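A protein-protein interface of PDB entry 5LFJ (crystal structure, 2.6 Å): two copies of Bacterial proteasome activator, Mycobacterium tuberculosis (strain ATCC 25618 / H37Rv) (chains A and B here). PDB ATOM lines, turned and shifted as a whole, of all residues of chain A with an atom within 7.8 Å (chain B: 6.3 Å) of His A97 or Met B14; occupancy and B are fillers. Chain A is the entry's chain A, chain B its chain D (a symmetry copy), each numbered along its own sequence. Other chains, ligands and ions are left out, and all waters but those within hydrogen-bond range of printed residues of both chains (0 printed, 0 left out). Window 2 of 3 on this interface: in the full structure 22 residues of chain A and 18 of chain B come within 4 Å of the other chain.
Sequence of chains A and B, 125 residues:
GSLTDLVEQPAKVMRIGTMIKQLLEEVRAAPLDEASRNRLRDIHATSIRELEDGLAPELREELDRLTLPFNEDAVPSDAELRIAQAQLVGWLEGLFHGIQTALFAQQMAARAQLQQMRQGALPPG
Met B14 touches one residue of chain A.
Of the printed residues of chain A, Thr B18 touches Gly A90 and Gly A94.
Printed residues of chain B within 4 Å of Leu A95: Arg B15 (3.7 Å).
Of the printed residues of chain A, Arg B15 touches Trp A91 and Leu A95.
The nearest printed residue of chain A that does not touch Arg B15 is Gly A94 (4.04 Å).
Position printed for both chains: 96.
Gly A90 touches Met B19.
Trp A91 touches Arg B15.
Trp A91 touches Met B19 (N to CA, 3.9 Å).
Leu A95 touches Arg B15.
Of the 14 printed residues of chain A, 5 touch a printed residue of chain B.
Along chain A the printed residues that touch a printed residue of chain B span positions 90 to 97.
Among the printed residues, 7 pairs touch across the chains.
Among the printed residues, no Asp or Glu carboxylate lies within 4 Å of a Lys or Arg side-chain nitrogen of the other chain.
O of His A97 lies within hydrogen-bond range of OG1 of Thr A101 (3.2 Å).
O of Arg B15 sits at hydrogen-bond distance from OG1 of Thr B18, 3.2 Å away.
The backbone NH (N) of Gly A94 lies close to the side-chain hydroxyl (OG1) of Thr B18 (3.1 Å).
A ring nitrogen (ND1) of His A97 lies within hydrogen-bond range of the side-chain sulfur (SD) of Met B14, at 3.8 Å.
The backbone carbonyl oxygen of Gly A90 is in hydrogen-bond range of the side-chain hydroxyl of Thr B18 (2.7 Å).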
ATOM      1  N   GLY A  90      -7.478   6.646 -32.215  1.00  0.00           N
ATOM      2  CA  GLY A  90      -7.340   5.868 -30.998  1.00  0.00           C
ATOM      3  C   GLY A  90      -5.937   5.948 -30.433  1.00  0.00           C
ATOM      4  O   GLY A  90      -5.746   6.147 -29.227  1.00  0.00           O
ATOM      5  N   TRP A  91      -4.936   5.853 -31.306  1.00  0.00           N
ATOM      6  CA  TRP A  91      -3.560   5.917 -30.846  1.00  0.00           C
ATOM      7  C   TRP A  91      -3.275   7.261 -30.165  1.00  0.00           C
ATOM      8  O   TRP A  91      -2.597   7.315 -29.132  1.00  0.00           O
ATOM      9  CB  TRP A  91      -2.622   5.682 -32.024  1.00  0.00           C
ATOM     10  CG  TRP A  91      -1.188   5.509 -31.647  1.00  0.00           C
ATOM     11  CD1 TRP A  91      -0.583   4.348 -31.242  1.00  0.00           C
ATOM     12  CD2 TRP A  91      -0.166   6.510 -31.660  1.00  0.00           C
ATOM     13  NE1 TRP A  91       0.750   4.576 -30.994  1.00  0.00           N
ATOM     14  CE2 TRP A  91       1.030   5.893 -31.245  1.00  0.00           C
ATOM     15  CE3 TRP A  91      -0.147   7.871 -31.974  1.00  0.00           C
ATOM     16  CZ2 TRP A  91       2.227   6.591 -31.130  1.00  0.00           C
ATOM     17  CZ3 TRP A  91       1.050   8.564 -31.854  1.00  0.00           C
ATOM     18  CH2 TRP A  91       2.216   7.923 -31.438  1.00  0.00           C
ATOM     19  N   LEU A  92      -3.814   8.350 -30.720  1.00  0.00           N
ATOM     20  CA  LEU A  92      -3.609   9.683 -30.161  1.00  0.00           C
ATOM     21  C   LEU A  92      -4.318   9.855 -28.818  1.00  0.00           C
ATOM     22  O   LEU A  92      -3.738  10.397 -27.859  1.00  0.00           O
ATOM     23  CB  LEU A  92      -4.095  10.723 -31.165  1.00  0.00           C
ATOM     24  CG  LEU A  92      -3.290  10.823 -32.463  1.00  0.00           C
ATOM     25  CD1 LEU A  92      -3.989  11.748 -33.459  1.00  0.00           C
ATOM     26  CD2 LEU A  92      -1.895  11.352 -32.152  1.00  0.00           C
ATOM     27  N   GLU A  93      -5.580   9.420 -28.732  1.00  0.00           N
ATOM     28  CA  GLU A  93      -6.296   9.521 -27.465  1.00  0.00           C
ATOM     29  C   GLU A  93      -5.592   8.739 -26.367  1.00  0.00           C
ATOM     30  O   GLU A  93      -5.522   9.198 -25.220  1.00  0.00           O
ATOM     31  CB  GLU A  93      -7.743   9.056 -27.610  1.00  0.00           C
ATOM     32  CG  GLU A  93      -8.596  10.019 -28.405  1.00  0.00           C
ATOM     33  CD  GLU A  93     -10.021   9.571 -28.501  1.00  0.00           C
ATOM     34  OE1 GLU A  93     -10.292   8.394 -28.186  1.00  0.00           O
ATOM     35  OE2 GLU A  93     -10.873  10.401 -28.875  1.00  0.00           O
ATOM     36  N   GLY A  94      -5.063   7.555 -26.693  1.00  0.00           N
ATOM     37  CA  GLY A  94      -4.275   6.825 -25.709  1.00  0.00           C
ATOM     38  C   GLY A  94      -3.020   7.572 -25.299  1.00  0.00           C
ATOM     39  O   GLY A  94      -2.672   7.623 -24.111  1.00  0.00           O
ATOM     40  N   LEU A  95      -2.338   8.182 -26.277  1.00  0.00           N
ATOM     41  CA  LEU A  95      -1.171   8.999 -25.965  1.00  0.00           C
ATOM     42  C   LEU A  95      -1.514  10.087 -24.945  1.00  0.00           C
ATOM     43  O   LEU A  95      -0.785  10.277 -23.958  1.00  0.00           O
ATOM     44  CB  LEU A  95      -0.614   9.612 -27.250  1.00  0.00           C
ATOM     45  CG  LEU A  95       0.611  10.530 -27.156  1.00  0.00           C
ATOM     46  CD1 LEU A  95       1.849   9.775 -26.664  1.00  0.00           C
ATOM     47  CD2 LEU A  95       0.871  11.198 -28.508  1.00  0.00           C
ATOM     48  N   PHE A  96      -2.667  10.754 -25.117  1.00  0.00           N
ATOM     49  CA  PHE A  96      -2.979  11.850 -24.205  1.00  0.00           C
ATOM     50  C   PHE A  96      -3.576  11.390 -22.885  1.00  0.00           C
ATOM     51  O   PHE A  96      -3.440  12.111 -21.893  1.00  0.00           O
ATOM     52  CB  PHE A  96      -3.954  12.879 -24.799  1.00  0.00           C
ATOM     53  CG  PHE A  96      -3.389  13.701 -25.928  1.00  0.00           C
ATOM     54  CD1 PHE A  96      -2.217  13.339 -26.570  1.00  0.00           C
ATOM     55  CD2 PHE A  96      -3.949  14.936 -26.228  1.00  0.00           C
ATOM     56  CE1 PHE A  96      -1.693  14.120 -27.589  1.00  0.00           C
ATOM     57  CE2 PHE A  96      -3.413  15.740 -27.226  1.00  0.00           C
ATOM     58  CZ  PHE A  96      -2.283  15.330 -27.908  1.00  0.00           C
ATOM     59  N   HIS A  97      -4.223  10.220 -22.826  1.00  0.00           N
ATOM     60  CA  HIS A  97      -4.586   9.699 -21.510  1.00  0.00           C
ATOM     61  C   HIS A  97      -3.337   9.301 -20.727  1.00  0.00           C
ATOM     62  O   HIS A  97      -3.340   9.342 -19.488  1.00  0.00           O
ATOM     63  CB  HIS A  97      -5.581   8.534 -21.640  1.00  0.00           C
ATOM     64  CG  HIS A  97      -6.280   8.183 -20.355  1.00  0.00           C
ATOM     65  ND1 HIS A  97      -7.036   7.039 -20.200  1.00  0.00           N
ATOM     66  CD2 HIS A  97      -6.346   8.837 -19.169  1.00  0.00           C
ATOM     67  CE1 HIS A  97      -7.534   7.003 -18.976  1.00  0.00           C
ATOM     68  NE2 HIS A  97      -7.129   8.082 -18.329  1.00  0.00           N
ATOM     69  N   GLY A  98      -2.260   8.937 -21.429  1.00  0.00           N
ATOM     70  CA  GLY A  98      -0.958   8.770 -20.805  1.00  0.00           C
ATOM     71  C   GLY A  98      -0.369  10.041 -20.213  1.00  0.00           C
ATOM     72  O   GLY A  98      -0.112  10.117 -18.994  1.00  0.00           O
ATOM     73  N   ILE A  99      -0.146  11.061 -21.052  1.00  0.00           N
ATOM     74  CA  ILE A  99       0.446  12.275 -20.483  1.00  0.00           C
ATOM     75  C   ILE A  99      -0.492  12.926 -19.471  1.00  0.00           C
ATOM     76  O   ILE A  99      -0.044  13.687 -18.609  1.00  0.00           O
ATOM     77  CB  ILE A  99       0.850  13.286 -21.579  1.00  0.00           C
ATOM     78  CG1 ILE A  99      -0.362  14.029 -22.159  1.00  0.00           C
ATOM     79  CG2 ILE A  99       1.623  12.579 -22.682  1.00  0.00           C
ATOM     80  CD1 ILE A  99      -0.540  15.467 -21.618  1.00  0.00           C
ATOM     81  N   GLN A 100      -1.792  12.636 -19.549  1.00  0.00           N
ATOM     82  CA  GLN A 100      -2.751  13.201 -18.609  1.00  0.00           C
ATOM     83  C   GLN A 100      -2.726  12.497 -17.253  1.00  0.00           C
ATOM     84  O   GLN A 100      -2.741  13.172 -16.215  1.00  0.00           O
ATOM     85  CB  GLN A 100      -4.149  13.170 -19.241  1.00  0.00           C
ATOM     86  CG  GLN A 100      -5.239  13.956 -18.516  1.00  0.00           C
ATOM     87  CD  GLN A 100      -6.592  13.929 -19.244  1.00  0.00           C
ATOM     88  OE1 GLN A 100      -6.683  13.490 -20.382  1.00  0.00           O
ATOM     89  NE2 GLN A 100      -7.660  14.276 -18.529  1.00  0.00           N
ATOM     90  N   THR A 101      -2.647  11.155 -17.223  1.00  0.00           N
ATOM     91  CA  THR A 101      -2.463  10.496 -15.927  1.00  0.00           C
ATOM     92  C   THR A 101      -1.118  10.863 -15.303  1.00  0.00           C
ATOM     93  O   THR A 101      -1.030  11.057 -14.077  1.00  0.00           O
ATOM     94  CB  THR A 101      -2.607   8.969 -16.062  1.00  0.00           C
ATOM     95  OG1 THR A 101      -3.954   8.642 -16.431  1.00  0.00           O
ATOM     96  CG2 THR A 101      -2.258   8.247 -14.743  1.00  0.00           C
ATOM     97  N   ALA A 102      -0.089  11.060 -16.134  1.00  0.00           N
ATOM     98  CA  ALA A 102       1.201  11.504 -15.612  1.00  0.00           C
ATOM     99  C   ALA A 102       1.101  12.901 -15.002  1.00  0.00           C
ATOM    100  O   ALA A 102       1.455  13.110 -13.835  1.00  0.00           O
ATOM    101  CB  ALA A 102       2.254  11.472 -16.722  1.00  0.00           C
ATOM    102  N   LEU A 103       0.642  13.877 -15.794  1.00  0.00           N
ATOM    103  CA  LEU A 103       0.529  15.250 -15.307  1.00  0.00           C
ATOM    104  C   LEU A 103      -0.330  15.348 -14.059  1.00  0.00           C
ATOM    105  O   LEU A 103       0.018  16.065 -13.116  1.00  0.00           O
ATOM    106  CB  LEU A 103      -0.041  16.156 -16.391  1.00  0.00           C
ATOM    107  CG  LEU A 103       0.963  16.498 -17.472  1.00  0.00           C
ATOM    108  CD1 LEU A 103       0.315  17.461 -18.398  1.00  0.00           C
ATOM    109  CD2 LEU A 103       2.210  17.070 -16.849  1.00  0.00           C
ATOM    110  N   GLN B   9       6.043  -0.868 -19.593  1.00  0.00           N
ATOM    111  CA  GLN B   9       5.850   0.439 -20.230  1.00  0.00           C
ATOM    112  C   GLN B   9       4.354   0.740 -20.253  1.00  0.00           C
ATOM    113  O   GLN B   9       3.682   0.527 -21.270  1.00  0.00           O
ATOM    114  CB  GLN B   9       6.449   0.454 -21.637  1.00  0.00           C
ATOM    115  CG  GLN B   9       7.867  -0.076 -21.703  1.00  0.00           C
ATOM    116  CD  GLN B   9       8.463  -0.024 -23.092  1.00  0.00           C
ATOM    117  OE1 GLN B   9       7.811   0.385 -24.053  1.00  0.00           O
ATOM    118  NE2 GLN B   9       9.699  -0.493 -23.217  1.00  0.00           N
ATOM    119  N   PRO B  10       3.798   1.259 -19.151  1.00  0.00           N
ATOM    120  CA  PRO B  10       2.329   1.371 -19.068  1.00  0.00           C
ATOM    121  C   PRO B  10       1.720   2.327 -20.079  1.00  0.00           C
ATOM    122  O   PRO B  10       0.648   2.040 -20.626  1.00  0.00           O
ATOM    123  CB  PRO B  10       2.101   1.866 -17.632  1.00  0.00           C
ATOM    124  CG  PRO B  10       3.331   1.469 -16.883  1.00  0.00           C
ATOM    125  CD  PRO B  10       4.454   1.574 -17.871  1.00  0.00           C
ATOM    126  N   ALA B  11       2.378   3.457 -20.354  1.00  0.00           N
ATOM    127  CA  ALA B  11       1.836   4.412 -21.315  1.00  0.00           C
ATOM    128  C   ALA B  11       1.675   3.771 -22.685  1.00  0.00           C
ATOM    129  O   ALA B  11       0.658   3.972 -23.359  1.00  0.00           O
ATOM    130  CB  ALA B  11       2.741   5.637 -21.412  1.00  0.00           C
ATOM    131  N   LYS B  12       2.677   2.999 -23.106  1.00  0.00           N
ATOM    132  CA  LYS B  12       2.648   2.358 -24.415  1.00  0.00           C
ATOM    133  C   LYS B  12       1.505   1.357 -24.514  1.00  0.00           C
ATOM    134  O   LYS B  12       0.796   1.309 -25.528  1.00  0.00           O
ATOM    135  CB  LYS B  12       3.986   1.676 -24.677  1.00  0.00           C
ATOM    136  CG  LYS B  12       4.089   0.983 -26.005  1.00  0.00           C
ATOM    137  CD  LYS B  12       5.482   0.431 -26.221  1.00  0.00           C
ATOM    138  CE  LYS B  12       5.580  -0.260 -27.554  1.00  0.00           C
ATOM    139  NZ  LYS B  12       6.937  -0.792 -27.812  1.00  0.00           N
ATOM    140  N   VAL B  13       1.322   0.537 -23.480  1.00  0.00           N
ATOM    141  CA  VAL B  13       0.252  -0.456 -23.506  1.00  0.00           C
ATOM    142  C   VAL B  13      -1.115   0.219 -23.511  1.00  0.00           C
ATOM    143  O   VAL B  13      -2.029  -0.208 -24.223  1.00  0.00           O
ATOM    144  CB  VAL B  13       0.413  -1.427 -22.333  1.00  0.00           C
ATOM    145  CG1 VAL B  13      -0.724  -2.442 -22.331  1.00  0.00           C
ATOM    146  CG2 VAL B  13       1.765  -2.108 -22.425  1.00  0.00           C
ATOM    147  N   MET B  14      -1.279   1.290 -22.736  1.00  0.00           N
ATOM    148  CA  MET B  14      -2.538   2.029 -22.796  1.00  0.00           C
ATOM    149  C   MET B  14      -2.785   2.563 -24.204  1.00  0.00           C
ATOM    150  O   MET B  14      -3.929   2.591 -24.684  1.00  0.00           O
ATOM    151  CB  MET B  14      -2.520   3.171 -21.786  1.00  0.00           C
ATOM    152  CG  MET B  14      -3.869   3.818 -21.538  1.00  0.00           C
ATOM    153  SD  MET B  14      -3.745   5.209 -20.384  1.00  0.00           S
ATOM    154  CE  MET B  14      -3.489   4.352 -18.829  1.00  0.00           C
ATOM    155  N   ARG B  15      -1.717   3.006 -24.876  1.00  0.00           N
ATOM    156  CA  ARG B  15      -1.846   3.629 -26.189  1.00  0.00           C
ATOM    157  C   ARG B  15      -2.221   2.607 -27.271  1.00  0.00           C
ATOM    158  O   ARG B  15      -3.209   2.791 -28.006  1.00  0.00           O
ATOM    159  CB  ARG B  15      -0.520   4.336 -26.489  1.00  0.00           C
ATOM    160  CG  ARG B  15      -0.378   5.016 -27.804  1.00  0.00           C
ATOM    161  CD  ARG B  15       0.917   5.837 -27.871  1.00  0.00           C
ATOM    162  NE  ARG B  15       2.142   5.075 -27.611  1.00  0.00           N
ATOM    163  CZ  ARG B  15       2.967   5.292 -26.578  1.00  0.00           C
ATOM    164  NH1 ARG B  15       2.733   6.276 -25.711  1.00  0.00           N
ATOM    165  NH2 ARG B  15       4.055   4.545 -26.428  1.00  0.00           N
ATOM    166  N   ILE B  16      -1.519   1.471 -27.311  1.00  0.00           N
ATOM    167  CA  ILE B  16      -1.922   0.385 -28.204  1.00  0.00           C
ATOM    168  C   ILE B  16      -3.354  -0.039 -27.909  1.00  0.00           C
ATOM    169  O   ILE B  16      -4.155  -0.276 -28.822  1.00  0.00           O
ATOM    170  CB  ILE B  16      -0.956  -0.809 -28.074  1.00  0.00           C
ATOM    171  CG1 ILE B  16       0.501  -0.388 -28.311  1.00  0.00           C
ATOM    172  CG2 ILE B  16      -1.339  -1.890 -29.057  1.00  0.00           C
ATOM    173  CD1 ILE B  16       0.768   0.223 -29.677  1.00  0.00           C
ATOM    174  N   GLY B  17      -3.703  -0.120 -26.627  1.00  0.00           N
ATOM    175  CA  GLY B  17      -5.032  -0.582 -26.263  1.00  0.00           C
ATOM    176  C   GLY B  17      -6.139   0.323 -26.755  1.00  0.00           C
ATOM    177  O   GLY B  17      -7.126  -0.147 -27.331  1.00  0.00           O
ATOM    178  N   THR B  18      -5.990   1.641 -26.568  1.00  0.00           N
ATOM    179  CA  THR B  18      -7.057   2.523 -27.042  1.00  0.00           C
ATOM    180  C   THR B  18      -7.115   2.529 -28.570  1.00  0.00           C
ATOM    181  O   THR B  18      -8.194   2.712 -29.151  1.00  0.00           O
ATOM    182  CB  THR B  18      -6.910   3.943 -26.479  1.00  0.00           C
ATOM    183  OG1 THR B  18      -5.731   4.548 -27.009  1.00  0.00           O
ATOM    184  CG2 THR B  18      -6.778   3.891 -24.972  1.00  0.00           C
ATOM    185  N   MET B  19      -5.968   2.350 -29.233  1.00  0.00           N
ATOM    186  CA  MET B  19      -5.981   2.197 -30.686  1.00  0.00           C
ATOM    187  C   MET B  19      -6.843   1.004 -31.098  1.00  0.00           C
ATOM    188  O   MET B  19      -7.686   1.098 -32.011  1.00  0.00           O
ATOM    189  CB  MET B  19      -4.561   2.003 -31.195  1.00  0.00           C
ATOM    190  CG  MET B  19      -4.494   1.855 -32.686  1.00  0.00           C
ATOM    191  SD  MET B  19      -2.850   1.433 -33.254  1.00  0.00           S
ATOM    192  CE  MET B  19      -2.801  -0.305 -32.812  1.00  0.00           C
ATOM    193  N   LEU B  51       2.581  -4.625 -27.938  1.00  0.00           N
ATOM    194  CA  LEU B  51       2.216  -4.999 -26.576  1.00  0.00           C
ATOM    195  C   LEU B  51       3.260  -5.917 -25.953  1.00  0.00           C
ATOM    196  O   LEU B  51       3.669  -5.717 -24.802  1.00  0.00           O
ATOM    197  CB  LEU B  51       0.864  -5.678 -26.553  1.00  0.00           C
ATOM    198  CG  LEU B  51      -0.342  -4.798 -26.782  1.00  0.00           C
ATOM    199  CD1 LEU B  51      -1.534  -5.731 -26.901  1.00  0.00           C
ATOM    200  CD2 LEU B  51      -0.495  -3.862 -25.615  1.00  0.00           C
ATOM    201  N   PHE B  96      -5.809  -3.689 -16.680  1.00  0.00           N
ATOM    202  CA  PHE B  96      -5.744  -2.403 -16.005  1.00  0.00           C
ATOM    203  C   PHE B  96      -6.711  -2.266 -14.840  1.00  0.00           C
ATOM    204  O   PHE B  96      -6.448  -1.447 -13.950  1.00  0.00           O
ATOM    205  CB  PHE B  96      -5.921  -1.258 -16.996  1.00  0.00           C
ATOM    206  CG  PHE B  96      -4.721  -1.054 -17.865  1.00  0.00           C
ATOM    207  CD1 PHE B  96      -3.550  -0.538 -17.315  1.00  0.00           C
ATOM    208  CD2 PHE B  96      -4.745  -1.355 -19.211  1.00  0.00           C
ATOM    209  CE1 PHE B  96      -2.422  -0.349 -18.088  1.00  0.00           C
ATOM    210  CE2 PHE B  96      -3.619  -1.161 -19.996  1.00  0.00           C
ATOM    211  CZ  PHE B  96      -2.456  -0.660 -19.435  1.00  0.00           C
